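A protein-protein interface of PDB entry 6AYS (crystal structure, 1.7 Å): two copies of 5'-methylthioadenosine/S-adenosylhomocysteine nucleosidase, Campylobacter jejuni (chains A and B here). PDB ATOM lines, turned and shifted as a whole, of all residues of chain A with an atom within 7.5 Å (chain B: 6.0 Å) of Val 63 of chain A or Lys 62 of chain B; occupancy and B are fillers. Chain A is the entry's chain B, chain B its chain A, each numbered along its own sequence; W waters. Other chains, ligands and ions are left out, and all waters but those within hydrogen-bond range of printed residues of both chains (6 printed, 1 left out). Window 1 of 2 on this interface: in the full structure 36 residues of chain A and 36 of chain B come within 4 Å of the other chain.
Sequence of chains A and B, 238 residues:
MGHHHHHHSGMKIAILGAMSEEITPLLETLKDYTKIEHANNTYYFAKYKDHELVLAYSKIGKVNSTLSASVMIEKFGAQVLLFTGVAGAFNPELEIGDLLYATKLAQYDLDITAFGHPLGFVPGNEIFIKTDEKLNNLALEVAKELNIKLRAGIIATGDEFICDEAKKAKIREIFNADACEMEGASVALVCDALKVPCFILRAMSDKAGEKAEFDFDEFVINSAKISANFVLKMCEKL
Hydrophobic or aromatic side chains of chain B within 4 Å of the printed part of chain A: Val 63, Leu 110 and Leu 189.
Hydrophobic or aromatic side chains of chain A that line the printed part of chain B: Val 63 and Leu 110.
Among the printed residues, 21 pairs touch across the chains.
Asp 109 of chain A touches Asp 159 of chain B, and with the chains exchanged Asp 159 of chain A touches Asp 109 of chain B.
Positions printed for both chains: 60, 61, 62, 63, 64, 65, 66, 67, 107, 109, 110, 158, 159, 182, 183 and 186.
Of the 21 pairs that touch across the chains among the printed residues, 19 have their exchanged pair printed and touching as well.
Val 63 of chain A touches five residues of chain B.
Lys 62 of chain B touches just these residues of chain A: Val 63 and Asp 159.
Of the printed residues of chain A, Thr 66 of chain B touches Val 63 (3.6 Å), Thr 66 (3.5 Å) and Leu 67 (3.8 Å).
Ser 65 of chain A touches none of the printed residues of chain B.
Met 182 of chain A touches none of the printed residues of chain B.
The nearest residue of chain B that does not touch Val 63 of chain A is Val 190 of chain B (5.2 Å).
The nearest printed residue of chain B that does not touch Leu 110 of chain A is Ile 60 of chain B (4.5 Å).
OD2 of Asp 109 of chain B is in hydrogen-bond range of N of Asp 159 of chain B (2.8 Å).
The side-chain hydroxyl (OG) of Ser 186 of chain A is in hydrogen-bond range of the side-chain hydroxyl (OG) of Ser 65 of chain A (3.0 Å).
Among the printed residues, merely in contact across the chains: Lys 62 of chain A with Val 63 of chain B (3.8 Å), Val 63 of chain A with Lys 62 of chain B (3.9 Å), Val 63 of chain A with Thr 66 of chain B (3.6 Å), Val 63 of chain A with Gln 107 of chain B (3.5 Å), Val 63 of chain A with Ser 186 of chain B (3.6 Å), Val 63 of chain A with Leu 189 of chain B (3.97 Å), Asn 64 of chain A with Leu 189 of chain B (3.9 Å), Thr 66 of chain A with Val 63 of chain B (3.6 Å), Thr 66 of chain A with Thr 66 of chain B (3.5 Å), Thr 66 of chain A with Leu 67 of chain B (3.8 Å), Leu 67 of chain A with Thr 66 of chain B (3.8 Å), Gln 107 of chain A with Val 63 of chain B (3.5 Å), Gln 107 of chain A with Asp 159 of chain B (3.9 Å), Leu 110 of chain A with Asp 159 of chain B (3.6 Å), Asp 159 of chain A with Gln 107 of chain B (3.8 Å), Asp 159 of chain A with Leu 110 of chain B (3.5 Å) and Ser 186 of chain A with Val 63 of chain B (3.7 Å).
Water W2 lies within hydrogen-bond range of OD2 of Asp 109 of chain B (2.8 Å) and O of Asp 109 of chain A (2.8 Å).
Water W4 bridges the side-chain amide nitrogen of Gln 107 of chain A and the side-chain amide oxygen of Asn 64 of chain B.
Water W5 lies within hydrogen-bond range of NE2 of Gln 107 of chain B (2.9 Å) and OD1 of Asn 64 of chain A (3.4 Å).
The side-chain amino group of Lys 62 of chain B is in salt-bridge range of the side-chain carboxylate of Asp 159 of chain A.
The side-chain carboxylate (OD2) of Asp 159 of chain B is in salt-bridge range of the side-chain amino group (NZ) of Lys 62 of chain A.
O of Asp 159 of chain B lies close to O of Asp 109 of chain A (3.2 Å).
O of Asp 109 of chain B lies close to O of Asp 159 of chain A.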
ATOM      1  N   SER A  58     -17.696 -29.529  26.958  1.00  0.00           N
ATOM      2  CA  SER A  58     -16.858 -28.381  26.609  1.00  0.00           C
ATOM      3  C   SER A  58     -15.667 -28.117  27.530  1.00  0.00           C
ATOM      4  O   SER A  58     -14.715 -27.464  27.133  1.00  0.00           O
ATOM      5  CB  SER A  58     -17.736 -27.129  26.558  1.00  0.00           C
ATOM      6  OG  SER A  58     -18.314 -26.874  27.820  1.00  0.00           O
ATOM      7  N   LYS A  59     -15.756 -28.644  28.741  1.00  0.00           N
ATOM      8  CA  LYS A  59     -15.027 -28.179  29.943  1.00  0.00           C
ATOM      9  C   LYS A  59     -15.747 -26.969  30.509  1.00  0.00           C
ATOM     10  O   LYS A  59     -16.574 -26.354  29.843  1.00  0.00           O
ATOM     11  CB  LYS A  59     -13.521 -27.940  29.701  1.00  0.00           C
ATOM     12  CG  LYS A  59     -12.808 -29.219  29.292  1.00  0.00           C
ATOM     13  CD  LYS A  59     -11.360 -28.965  28.892  1.00  0.00           C
ATOM     14  CE  LYS A  59     -11.249 -28.471  27.456  1.00  0.00           C
ATOM     15  NZ  LYS A  59      -9.805 -28.364  27.083  1.00  0.00           N
ATOM     16  N   ILE A  60     -15.441 -26.649  31.753  1.00  0.00           N
ATOM     17  CA  ILE A  60     -16.273 -25.744  32.538  1.00  0.00           C
ATOM     18  C   ILE A  60     -16.141 -24.292  32.097  1.00  0.00           C
ATOM     19  O   ILE A  60     -15.052 -23.821  31.798  1.00  0.00           O
ATOM     20  CB  ILE A  60     -15.944 -25.889  34.039  1.00  0.00           C
ATOM     21  CG1 ILE A  60     -16.380 -27.283  34.509  1.00  0.00           C
ATOM     22  CG2 ILE A  60     -16.596 -24.791  34.885  1.00  0.00           C
ATOM     23  CD1 ILE A  60     -15.778 -27.697  35.837  1.00  0.00           C
ATOM     24  N   GLY A  61     -17.277 -23.601  32.065  1.00  0.00           N
ATOM     25  CA  GLY A  61     -17.296 -22.139  32.010  1.00  0.00           C
ATOM     26  C   GLY A  61     -17.668 -21.543  30.675  1.00  0.00           C
ATOM     27  O   GLY A  61     -17.878 -22.249  29.680  1.00  0.00           O
ATOM     28  N   LYS A  62     -17.736 -20.217  30.659  1.00  0.00           N
ATOM     29  CA  LYS A  62     -18.295 -19.486  29.518  1.00  0.00           C
ATOM     30  C   LYS A  62     -17.440 -19.583  28.258  1.00  0.00           C
ATOM     31  O   LYS A  62     -17.967 -19.790  27.168  1.00  0.00           O
ATOM     32  CB  LYS A  62     -18.509 -18.025  29.883  1.00  0.00           C
ATOM     33  CG  LYS A  62     -19.573 -17.815  30.937  1.00  0.00           C
ATOM     34  CD  LYS A  62     -20.032 -16.360  31.034  1.00  0.00           C
ATOM     35  CE  LYS A  62     -18.886 -15.414  31.353  1.00  0.00           C
ATOM     36  NZ  LYS A  62     -19.378 -14.032  31.573  1.00  0.00           N
ATOM     37  N   VAL A  63     -16.127 -19.409  28.406  1.00  0.00           N
ATOM     38  CA  VAL A  63     -15.227 -19.439  27.263  1.00  0.00           C
ATOM     39  C   VAL A  63     -15.208 -20.831  26.632  1.00  0.00           C
ATOM     40  O   VAL A  63     -15.372 -20.966  25.408  1.00  0.00           O
ATOM     41  CB  VAL A  63     -13.799 -18.965  27.632  1.00  0.00           C
ATOM     42  CG1 VAL A  63     -12.819 -19.204  26.482  1.00  0.00           C
ATOM     43  CG2 VAL A  63     -13.833 -17.477  27.987  1.00  0.00           C
ATOM     44  N   ASN A  64     -15.015 -21.859  27.463  1.00  0.00           N
ATOM     45  CA  ASN A  64     -14.966 -23.234  26.965  1.00  0.00           C
ATOM     46  C   ASN A  64     -16.261 -23.630  26.241  1.00  0.00           C
ATOM     47  O   ASN A  64     -16.217 -24.223  25.150  1.00  0.00           O
ATOM     48  CB  ASN A  64     -14.676 -24.226  28.103  1.00  0.00           C
ATOM     49  CG  ASN A  64     -13.233 -24.160  28.592  1.00  0.00           C
ATOM     50  OD1 ASN A  64     -12.321 -23.837  27.837  1.00  0.00           O
ATOM     51  ND2 ASN A  64     -13.026 -24.441  29.876  1.00  0.00           N
ATOM     52  N   SER A  65     -17.404 -23.293  26.838  1.00  0.00           N
ATOM     53  CA  SER A  65     -18.705 -23.635  26.245  1.00  0.00           C
ATOM     54  C   SER A  65     -18.989 -22.847  24.975  1.00  0.00           C
ATOM     55  O   SER A  65     -19.551 -23.393  24.019  1.00  0.00           O
ATOM     56  CB  SER A  65     -19.836 -23.483  27.274  1.00  0.00           C
ATOM     57  OG  SER A  65     -20.000 -22.145  27.716  1.00  0.00           O
ATOM     58  N   THR A  66     -18.574 -21.580  24.937  1.00  0.00           N
ATOM     59  CA  THR A  66     -18.689 -20.759  23.720  1.00  0.00           C
ATOM     60  C   THR A  66     -17.913 -21.400  22.571  1.00  0.00           C
ATOM     61  O   THR A  66     -18.431 -21.526  21.461  1.00  0.00           O
ATOM     62  CB  THR A  66     -18.179 -19.329  23.951  1.00  0.00           C
ATOM     63  OG1 THR A  66     -18.951 -18.715  24.982  1.00  0.00           O
ATOM     64  CG2 THR A  66     -18.302 -18.476  22.698  1.00  0.00           C
ATOM     65  N   LEU A  67     -16.674 -21.796  22.850  1.00  0.00           N
ATOM     66  CA  LEU A  67     -15.829 -22.418  21.836  1.00  0.00           C
ATOM     67  C   LEU A  67     -16.471 -23.697  21.297  1.00  0.00           C
ATOM     68  O   LEU A  67     -16.547 -23.881  20.081  1.00  0.00           O
ATOM     69  CB  LEU A  67     -14.430 -22.705  22.393  1.00  0.00           C
ATOM     70  CG  LEU A  67     -13.458 -23.491  21.504  1.00  0.00           C
ATOM     71  CD1 LEU A  67     -13.237 -22.787  20.177  1.00  0.00           C
ATOM     72  CD2 LEU A  67     -12.167 -23.727  22.273  1.00  0.00           C
ATOM     73  N   SER A  68     -16.938 -24.573  22.195  1.00  0.00           N
ATOM     74  CA  SER A  68     -17.536 -25.844  21.763  1.00  0.00           C
ATOM     75  C   SER A  68     -18.808 -25.652  20.932  1.00  0.00           C
ATOM     76  O   SER A  68     -18.971 -26.302  19.904  1.00  0.00           O
ATOM     77  CB  SER A  68     -17.821 -26.766  22.931  1.00  0.00           C
ATOM     78  OG  SER A  68     -16.615 -27.349  23.415  1.00  0.00           O
ATOM     79  N   ALA A  69     -19.694 -24.755  21.362  1.00  0.00           N
ATOM     80  CA  ALA A  69     -20.895 -24.440  20.569  1.00  0.00           C
ATOM     81  C   ALA A  69     -20.513 -23.910  19.179  1.00  0.00           C
ATOM     82  O   ALA A  69     -21.102 -24.325  18.174  1.00  0.00           O
ATOM     83  CB  ALA A  69     -21.780 -23.436  21.293  1.00  0.00           C
ATOM     84  N   GLN A 107     -25.869 -13.197  31.527  1.00  0.00           N
ATOM     85  CA  GLN A 107     -24.554 -13.293  32.180  1.00  0.00           C
ATOM     86  C   GLN A 107     -24.514 -12.335  33.360  1.00  0.00           C
ATOM     87  O   GLN A 107     -24.392 -11.118  33.165  1.00  0.00           O
ATOM     88  CB  GLN A 107     -23.429 -12.970  31.192  1.00  0.00           C
ATOM     89  CG  GLN A 107     -23.255 -13.989  30.085  1.00  0.00           C
ATOM     90  CD  GLN A 107     -22.259 -13.546  29.043  1.00  0.00           C
ATOM     91  OE1 GLN A 107     -21.067 -13.403  29.335  1.00  0.00           O
ATOM     92  NE2 GLN A 107     -22.750 -13.316  27.804  1.00  0.00           N
ATOM     93  N   ASP A 109     -22.159 -11.834  35.497  1.00  0.00           N
ATOM     94  CA  ASP A 109     -20.814 -11.324  35.753  1.00  0.00           C
ATOM     95  C   ASP A 109     -20.224 -10.539  34.571  1.00  0.00           C
ATOM     96  O   ASP A 109     -19.019 -10.266  34.543  1.00  0.00           O
ATOM     97  CB  ASP A 109     -19.876 -12.462  36.186  1.00  0.00           C
ATOM     98  CG  ASP A 109     -19.660 -13.515  35.100  1.00  0.00           C
ATOM     99  OD1 ASP A 109     -20.365 -13.493  34.068  1.00  0.00           O
ATOM    100  OD2 ASP A 109     -18.777 -14.379  35.294  1.00  0.00           O
ATOM    101  N   LEU A 110     -21.069 -10.177  33.609  1.00  0.00           N
ATOM    102  CA  LEU A 110     -20.672  -9.299  32.514  1.00  0.00           C
ATOM    103  C   LEU A 110     -21.023  -7.890  32.973  1.00  0.00           C
ATOM    104  O   LEU A 110     -22.195  -7.540  33.077  1.00  0.00           O
ATOM    105  CB  LEU A 110     -21.391  -9.687  31.223  1.00  0.00           C
ATOM    106  CG  LEU A 110     -21.048  -8.900  29.954  1.00  0.00           C
ATOM    107  CD1 LEU A 110     -19.560  -8.896  29.661  1.00  0.00           C
ATOM    108  CD2 LEU A 110     -21.817  -9.482  28.777  1.00  0.00           C
ATOM    109  N   GLY A 158     -22.618 -17.417  34.861  1.00  0.00           N
ATOM    110  CA  GLY A 158     -21.378 -16.698  35.112  1.00  0.00           C
ATOM    111  C   GLY A 158     -20.270 -17.680  35.403  1.00  0.00           C
ATOM    112  O   GLY A 158     -20.523 -18.872  35.519  1.00  0.00           O
ATOM    113  N   ASP A 159     -19.047 -17.180  35.541  1.00  0.00           N
ATOM    114  CA  ASP A 159     -17.872 -18.044  35.672  1.00  0.00           C
ATOM    115  C   ASP A 159     -17.457 -18.337  37.117  1.00  0.00           C
ATOM    116  O   ASP A 159     -16.300 -18.662  37.372  1.00  0.00           O
ATOM    117  CB  ASP A 159     -16.708 -17.472  34.844  1.00  0.00           C
ATOM    118  CG  ASP A 159     -16.668 -18.025  33.422  1.00  0.00           C
ATOM    119  OD1 ASP A 159     -17.268 -19.097  33.158  1.00  0.00           O
ATOM    120  OD2 ASP A 159     -16.012 -17.396  32.577  1.00  0.00           O
ATOM    121  N   MET A 182     -22.731 -22.162  34.557  1.00  0.00           N
ATOM    122  CA  MET A 182     -21.532 -21.484  34.064  1.00  0.00           C
ATOM    123  C   MET A 182     -21.370 -21.546  32.544  1.00  0.00           C
ATOM    124  O   MET A 182     -20.319 -21.179  32.028  1.00  0.00           O
ATOM    125  CB  MET A 182     -20.300 -22.058  34.785  1.00  0.00           C
ATOM    126  CG  MET A 182     -20.387 -21.962  36.313  1.00  0.00           C
ATOM    127  SD  MET A 182     -19.083 -22.801  37.233  1.00  0.00           S
ATOM    128  CE  MET A 182     -17.662 -21.804  36.841  1.00  0.00           C
ATOM    129  N   GLU A 183     -22.412 -21.972  31.832  1.00  0.00           N
ATOM    130  CA  GLU A 183     -22.333 -22.201  30.379  1.00  0.00           C
ATOM    131  C   GLU A 183     -23.564 -21.826  29.536  1.00  0.00           C
ATOM    132  O   GLU A 183     -23.448 -21.726  28.312  1.00  0.00           O
ATOM    133  CB  GLU A 183     -22.024 -23.679  30.096  1.00  0.00           C
ATOM    134  CG  GLU A 183     -20.759 -24.230  30.744  1.00  0.00           C
ATOM    135  CD  GLU A 183     -20.895 -24.675  32.192  1.00  0.00           C
ATOM    136  OE1 GLU A 183     -22.024 -24.832  32.708  1.00  0.00           O
ATOM    137  OE2 GLU A 183     -19.840 -24.879  32.821  1.00  0.00           O
ATOM    138  N   SER A 186     -23.888 -18.278  27.463  1.00  0.00           N
ATOM    139  CA  SER A 186     -22.853 -18.247  26.435  1.00  0.00           C
ATOM    140  C   SER A 186     -23.214 -19.158  25.253  1.00  0.00           C
ATOM    141  O   SER A 186     -23.108 -18.754  24.098  1.00  0.00           O
ATOM    142  CB  SER A 186     -21.484 -18.633  27.030  1.00  0.00           C
ATOM    143  OG  SER A 186     -21.597 -19.661  27.987  1.00  0.00           O
ATOM    144  N   ILE B  60     -17.905  -6.383  23.381  1.00  0.00           N
ATOM    145  CA  ILE B  60     -17.105  -6.449  24.601  1.00  0.00           C
ATOM    146  C   ILE B  60     -17.235  -7.789  25.311  1.00  0.00           C
ATOM    147  O   ILE B  60     -18.323  -8.360  25.394  1.00  0.00           O
ATOM    148  CB  ILE B  60     -17.509  -5.294  25.544  1.00  0.00           C
ATOM    149  CG1 ILE B  60     -17.095  -3.958  24.908  1.00  0.00           C
ATOM    150  CG2 ILE B  60     -16.895  -5.451  26.931  1.00  0.00           C
ATOM    151  CD1 ILE B  60     -17.781  -2.759  25.526  1.00  0.00           C
ATOM    152  N   GLY B  61     -16.105  -8.274  25.822  1.00  0.00           N
ATOM    153  CA  GLY B  61     -16.104  -9.347  26.815  1.00  0.00           C
ATOM    154  C   GLY B  61     -15.689 -10.711  26.300  1.00  0.00           C
ATOM    155  O   GLY B  61     -15.428 -10.909  25.108  1.00  0.00           O
ATOM    156  N   LYS B  62     -15.649 -11.659  27.224  1.00  0.00           N
ATOM    157  CA  LYS B  62     -15.053 -12.973  26.957  1.00  0.00           C
ATOM    158  C   LYS B  62     -15.853 -13.808  25.969  1.00  0.00           C
ATOM    159  O   LYS B  62     -15.271 -14.423  25.073  1.00  0.00           O
ATOM    160  CB  LYS B  62     -14.884 -13.749  28.259  1.00  0.00           C
ATOM    161  CG  LYS B  62     -13.872 -13.132  29.203  1.00  0.00           C
ATOM    162  CD  LYS B  62     -13.450 -14.086  30.308  1.00  0.00           C
ATOM    163  CE  LYS B  62     -14.635 -14.565  31.148  1.00  0.00           C
ATOM    164  NZ  LYS B  62     -14.181 -15.383  32.304  1.00  0.00           N
ATOM    165  N   VAL B  63     -17.174 -13.852  26.138  1.00  0.00           N
ATOM    166  CA  VAL B  63     -18.020 -14.659  25.261  1.00  0.00           C
ATOM    167  C   VAL B  63     -17.988 -14.116  23.841  1.00  0.00           C
ATOM    168  O   VAL B  63     -17.765 -14.880  22.888  1.00  0.00           O
ATOM    169  CB  VAL B  63     -19.475 -14.766  25.794  1.00  0.00           C
ATOM    170  CG1 VAL B  63     -20.401 -15.412  24.774  1.00  0.00           C
ATOM    171  CG2 VAL B  63     -19.491 -15.555  27.098  1.00  0.00           C
ATOM    172  N   ASN B  64     -18.198 -12.809  23.694  1.00  0.00           N
ATOM    173  CA  ASN B  64     -18.199 -12.177  22.367  1.00  0.00           C
ATOM    174  C   ASN B  64     -16.866 -12.391  21.637  1.00  0.00           C
ATOM    175  O   ASN B  64     -16.852 -12.747  20.448  1.00  0.00           O
ATOM    176  CB  ASN B  64     -18.528 -10.688  22.466  1.00  0.00           C
ATOM    177  CG  ASN B  64     -19.992 -10.424  22.801  1.00  0.00           C
ATOM    178  OD1 ASN B  64     -20.883 -11.212  22.444  1.00  0.00           O
ATOM    179  ND2 ASN B  64     -20.255  -9.322  23.516  1.00  0.00           N
ATOM    180  N   SER B  65     -15.756 -12.189  22.341  1.00  0.00           N
ATOM    181  CA  SER B  65     -14.425 -12.334  21.738  1.00  0.00           C
ATOM    182  C   SER B  65     -14.099 -13.792  21.412  1.00  0.00           C
ATOM    183  O   SER B  65     -13.487 -14.072  20.381  1.00  0.00           O
ATOM    184  CB  SER B  65     -13.342 -11.699  22.620  1.00  0.00           C
ATOM    185  OG  SER B  65     -13.221 -12.332  23.887  1.00  0.00           O
ATOM    186  N   THR B  66     -14.533 -14.725  22.266  1.00  0.00           N
ATOM    187  CA  THR B  66     -14.376 -16.160  21.990  1.00  0.00           C
ATOM    188  C   THR B  66     -15.097 -16.535  20.699  1.00  0.00           C
ATOM    189  O   THR B  66     -14.531 -17.223  19.851  1.00  0.00           O
ATOM    190  CB  THR B  66     -14.927 -17.020  23.146  1.00  0.00           C
ATOM    191  OG1 THR B  66     -14.212 -16.714  24.340  1.00  0.00           O
ATOM    192  CG2 THR B  66     -14.768 -18.511  22.867  1.00  0.00           C
ATOM    193  N   LEU B  67     -16.338 -16.080  20.560  1.00  0.00           N
ATOM    194  CA  LEU B  67     -17.127 -16.374  19.369  1.00  0.00           C
ATOM    195  C   LEU B  67     -16.445 -15.840  18.115  1.00  0.00           C
ATOM    196  O   LEU B  67     -16.307 -16.578  17.131  1.00  0.00           O
ATOM    197  CB  LEU B  67     -18.546 -15.803  19.495  1.00  0.00           C
ATOM    198  CG  LEU B  67     -19.462 -15.936  18.275  1.00  0.00           C
ATOM    199  CD1 LEU B  67     -19.624 -17.389  17.842  1.00  0.00           C
ATOM    200  CD2 LEU B  67     -20.786 -15.251  18.554  1.00  0.00           C
ATOM    201  N   GLN B 107      -7.708 -15.891  33.130  1.00  0.00           N
ATOM    202  CA  GLN B 107      -9.043 -15.384  33.458  1.00  0.00           C
ATOM    203  C   GLN B 107      -9.159 -15.230  34.973  1.00  0.00           C
ATOM    204  O   GLN B 107      -9.296 -16.233  35.691  1.00  0.00           O
ATOM    205  CB  GLN B 107     -10.125 -16.333  32.946  1.00  0.00           C
ATOM    206  CG  GLN B 107     -10.241 -16.388  31.436  1.00  0.00           C
ATOM    207  CD  GLN B 107     -11.207 -17.458  30.975  1.00  0.00           C
ATOM    208  OE1 GLN B 107     -12.407 -17.372  31.235  1.00  0.00           O
ATOM    209  NE2 GLN B 107     -10.683 -18.481  30.281  1.00  0.00           N
ATOM    210  N   ASP B 109     -11.604 -14.112  36.742  1.00  0.00           N
ATOM    211  CA  ASP B 109     -12.969 -14.311  37.226  1.00  0.00           C
ATOM    212  C   ASP B 109     -13.526 -15.708  36.929  1.00  0.00           C
ATOM    213  O   ASP B 109     -14.728 -15.937  37.062  1.00  0.00           O
ATOM    214  CB  ASP B 109     -13.902 -13.214  36.677  1.00  0.00           C
ATOM    215  CG  ASP B 109     -14.047 -13.244  35.166  1.00  0.00           C
ATOM    216  OD1 ASP B 109     -13.301 -13.981  34.484  1.00  0.00           O
ATOM    217  OD2 ASP B 109     -14.920 -12.505  34.654  1.00  0.00           O
ATOM    218  N   LEU B 110     -12.648 -16.634  36.541  1.00  0.00           N
ATOM    219  CA  LEU B 110     -13.018 -18.031  36.372  1.00  0.00           C
ATOM    220  C   LEU B 110     -12.698 -18.694  37.704  1.00  0.00           C
ATOM    221  O   LEU B 110     -11.530 -18.851  38.062  1.00  0.00           O
ATOM    222  CB  LEU B 110     -12.246 -18.654  35.208  1.00  0.00           C
ATOM    223  CG  LEU B 110     -12.538 -20.115  34.857  1.00  0.00           C
ATOM    224  CD1 LEU B 110     -14.018 -20.344  34.594  1.00  0.00           C
ATOM    225  CD2 LEU B 110     -11.711 -20.520  33.650  1.00  0.00           C
ATOM    226  N   THR B 157      -7.510 -11.225  32.318  1.00  0.00           N
ATOM    227  CA  THR B 157      -8.746 -11.006  31.576  1.00  0.00           C
ATOM    228  C   THR B 157      -9.945 -11.397  32.424  1.00  0.00           C
ATOM    229  O   THR B 157      -9.915 -12.400  33.127  1.00  0.00           O
ATOM    230  CB  THR B 157      -8.745 -11.862  30.302  1.00  0.00           C
ATOM    231  OG1 THR B 157      -7.697 -11.414  29.444  1.00  0.00           O
ATOM    232  CG2 THR B 157     -10.096 -11.787  29.554  1.00  0.00           C
ATOM    233  N   GLY B 158     -11.002 -10.595  32.362  1.00  0.00           N
ATOM    234  CA  GLY B 158     -12.271 -10.955  32.997  1.00  0.00           C
ATOM    235  C   GLY B 158     -13.367 -10.069  32.465  1.00  0.00           C
ATOM    236  O   GLY B 158     -13.092  -9.132  31.717  1.00  0.00           O
ATOM    237  N   ASP B 159     -14.601 -10.342  32.866  1.00  0.00           N
ATOM    238  CA  ASP B 159     -15.765  -9.651  32.295  1.00  0.00           C
ATOM    239  C   ASP B 159     -16.230  -8.423  33.085  1.00  0.00           C
ATOM    240  O   ASP B 159     -17.386  -8.032  32.983  1.00  0.00           O
ATOM    241  CB  ASP B 159     -16.906 -10.661  32.071  1.00  0.00           C
ATOM    242  CG  ASP B 159     -16.880 -11.282  30.678  1.00  0.00           C
ATOM    243  OD1 ASP B 159     -16.251 -10.703  29.759  1.00  0.00           O
ATOM    244  OD2 ASP B 159     -17.514 -12.340  30.497  1.00  0.00           O
ATOM    245  N   MET B 182     -10.770  -7.443  28.819  1.00  0.00           N
ATOM    246  CA  MET B 182     -11.963  -8.290  28.896  1.00  0.00           C
ATOM    247  C   MET B 182     -12.062  -9.324  27.772  1.00  0.00           C
ATOM    248  O   MET B 182     -13.103  -9.967  27.626  1.00  0.00           O
ATOM    249  CB  MET B 182     -13.211  -7.394  28.949  1.00  0.00           C
ATOM    250  CG  MET B 182     -13.195  -6.381  30.081  1.00  0.00           C
ATOM    251  SD  MET B 182     -14.507  -5.155  30.070  1.00  0.00           S
ATOM    252  CE  MET B 182     -15.947  -6.170  30.442  1.00  0.00           C
ATOM    253  N   GLU B 183     -10.982  -9.503  27.011  1.00  0.00           N
ATOM    254  CA  GLU B 183     -10.996 -10.368  25.819  1.00  0.00           C
ATOM    255  C   GLU B 183      -9.738 -11.211  25.541  1.00  0.00           C
ATOM    256  O   GLU B 183      -9.808 -12.152  24.751  1.00  0.00           O
ATOM    257  CB  GLU B 183     -11.270  -9.529  24.574  1.00  0.00           C
ATOM    258  CG  GLU B 183     -12.556  -8.705  24.585  1.00  0.00           C
ATOM    259  CD  GLU B 183     -12.467  -7.363  25.298  1.00  0.00           C
ATOM    260  OE1 GLU B 183     -11.350  -6.865  25.598  1.00  0.00           O
ATOM    261  OE2 GLU B 183     -13.556  -6.795  25.559  1.00  0.00           O
ATOM    262  N   ALA B 185      -7.422 -13.322  27.218  1.00  0.00           N
ATOM    263  CA  ALA B 185      -7.242 -14.725  27.615  1.00  0.00           C
ATOM    264  C   ALA B 185      -8.167 -15.640  26.838  1.00  0.00           C
ATOM    265  O   ALA B 185      -7.762 -16.735  26.450  1.00  0.00           O
ATOM    266  CB  ALA B 185      -7.450 -14.905  29.106  1.00  0.00           C
ATOM    267  N   SER B 186      -9.398 -15.180  26.603  1.00  0.00           N
ATOM    268  CA  SER B 186     -10.388 -15.951  25.857  1.00  0.00           C
ATOM    269  C   SER B 186      -9.962 -16.134  24.393  1.00  0.00           C
ATOM    270  O   SER B 186     -10.023 -17.244  23.859  1.00  0.00           O
ATOM    271  CB  SER B 186     -11.772 -15.277  25.947  1.00  0.00           C
ATOM    272  OG  SER B 186     -11.683 -13.869  25.903  1.00  0.00           O
ATOM    273  N   VAL B 187      -9.505 -15.059  23.760  1.00  0.00           N
ATOM    274  CA  VAL B 187      -9.025 -15.134  22.370  1.00  0.00           C
ATOM    275  C   VAL B 187      -7.789 -16.046  22.274  1.00  0.00           C
ATOM    276  O   VAL B 187      -7.707 -16.897  21.386  1.00  0.00           O
ATOM    277  CB  VAL B 187      -8.722 -13.737  21.791  1.00  0.00           C
ATOM    278  CG1 VAL B 187      -7.991 -13.822  20.460  1.00  0.00           C
ATOM    279  CG2 VAL B 187     -10.013 -12.944  21.628  1.00  0.00           C
ATOM    280  N   LEU B 189      -6.914 -18.452  24.283  1.00  0.00           N
ATOM    281  CA  LEU B 189      -7.360 -19.830  24.513  1.00  0.00           C
ATOM    282  C   LEU B 189      -7.902 -20.460  23.235  1.00  0.00           C
ATOM    283  O   LEU B 189      -7.528 -21.589  22.894  1.00  0.00           O
ATOM    284  CB  LEU B 189      -8.406 -19.876  25.626  1.00  0.00           C
ATOM    285  CG  LEU B 189      -8.993 -21.258  26.009  1.00  0.00           C
ATOM    286  CD1 LEU B 189      -9.490 -21.231  27.451  1.00  0.00           C
ATOM    287  CD2 LEU B 189     -10.096 -21.724  25.064  1.00  0.00           C
ATOM    288  N   VAL B 190      -8.778 -19.734  22.531  1.00  0.00           N
ATOM    289  CA  VAL B 190      -9.338 -20.223  21.270  1.00  0.00           C
ATOM    290  C   VAL B 190      -8.228 -20.545  20.282  1.00  0.00           C
ATOM    291  O   VAL B 190      -8.200 -21.633  19.699  1.00  0.00           O
ATOM    292  CB  VAL B 190     -10.316 -19.208  20.630  1.00  0.00           C
ATOM    293  CG1 VAL B 190     -10.708 -19.623  19.209  1.00  0.00           C
ATOM    294  CG2 VAL B 190     -11.570 -19.032  21.480  1.00  0.00           C
HETATM  295  O   HOH W   1     -17.146 -14.772  37.519  1.00  0.00           O
HETATM  296  O   HOH W   2     -16.566 -10.627  35.920  1.00  0.00           O
HETATM  297  O   HOH W   3     -14.621 -18.936  31.006  1.00  0.00           O
HETATM  298  O   HOH W   4     -21.622 -11.686  25.731  1.00  0.00           O
HETATM  299  O   HOH W   5     -11.722 -21.169  29.829  1.00  0.00           O
HETATM  300  O   HOH W   6     -18.754 -12.457  28.221  1.00  0.00           O
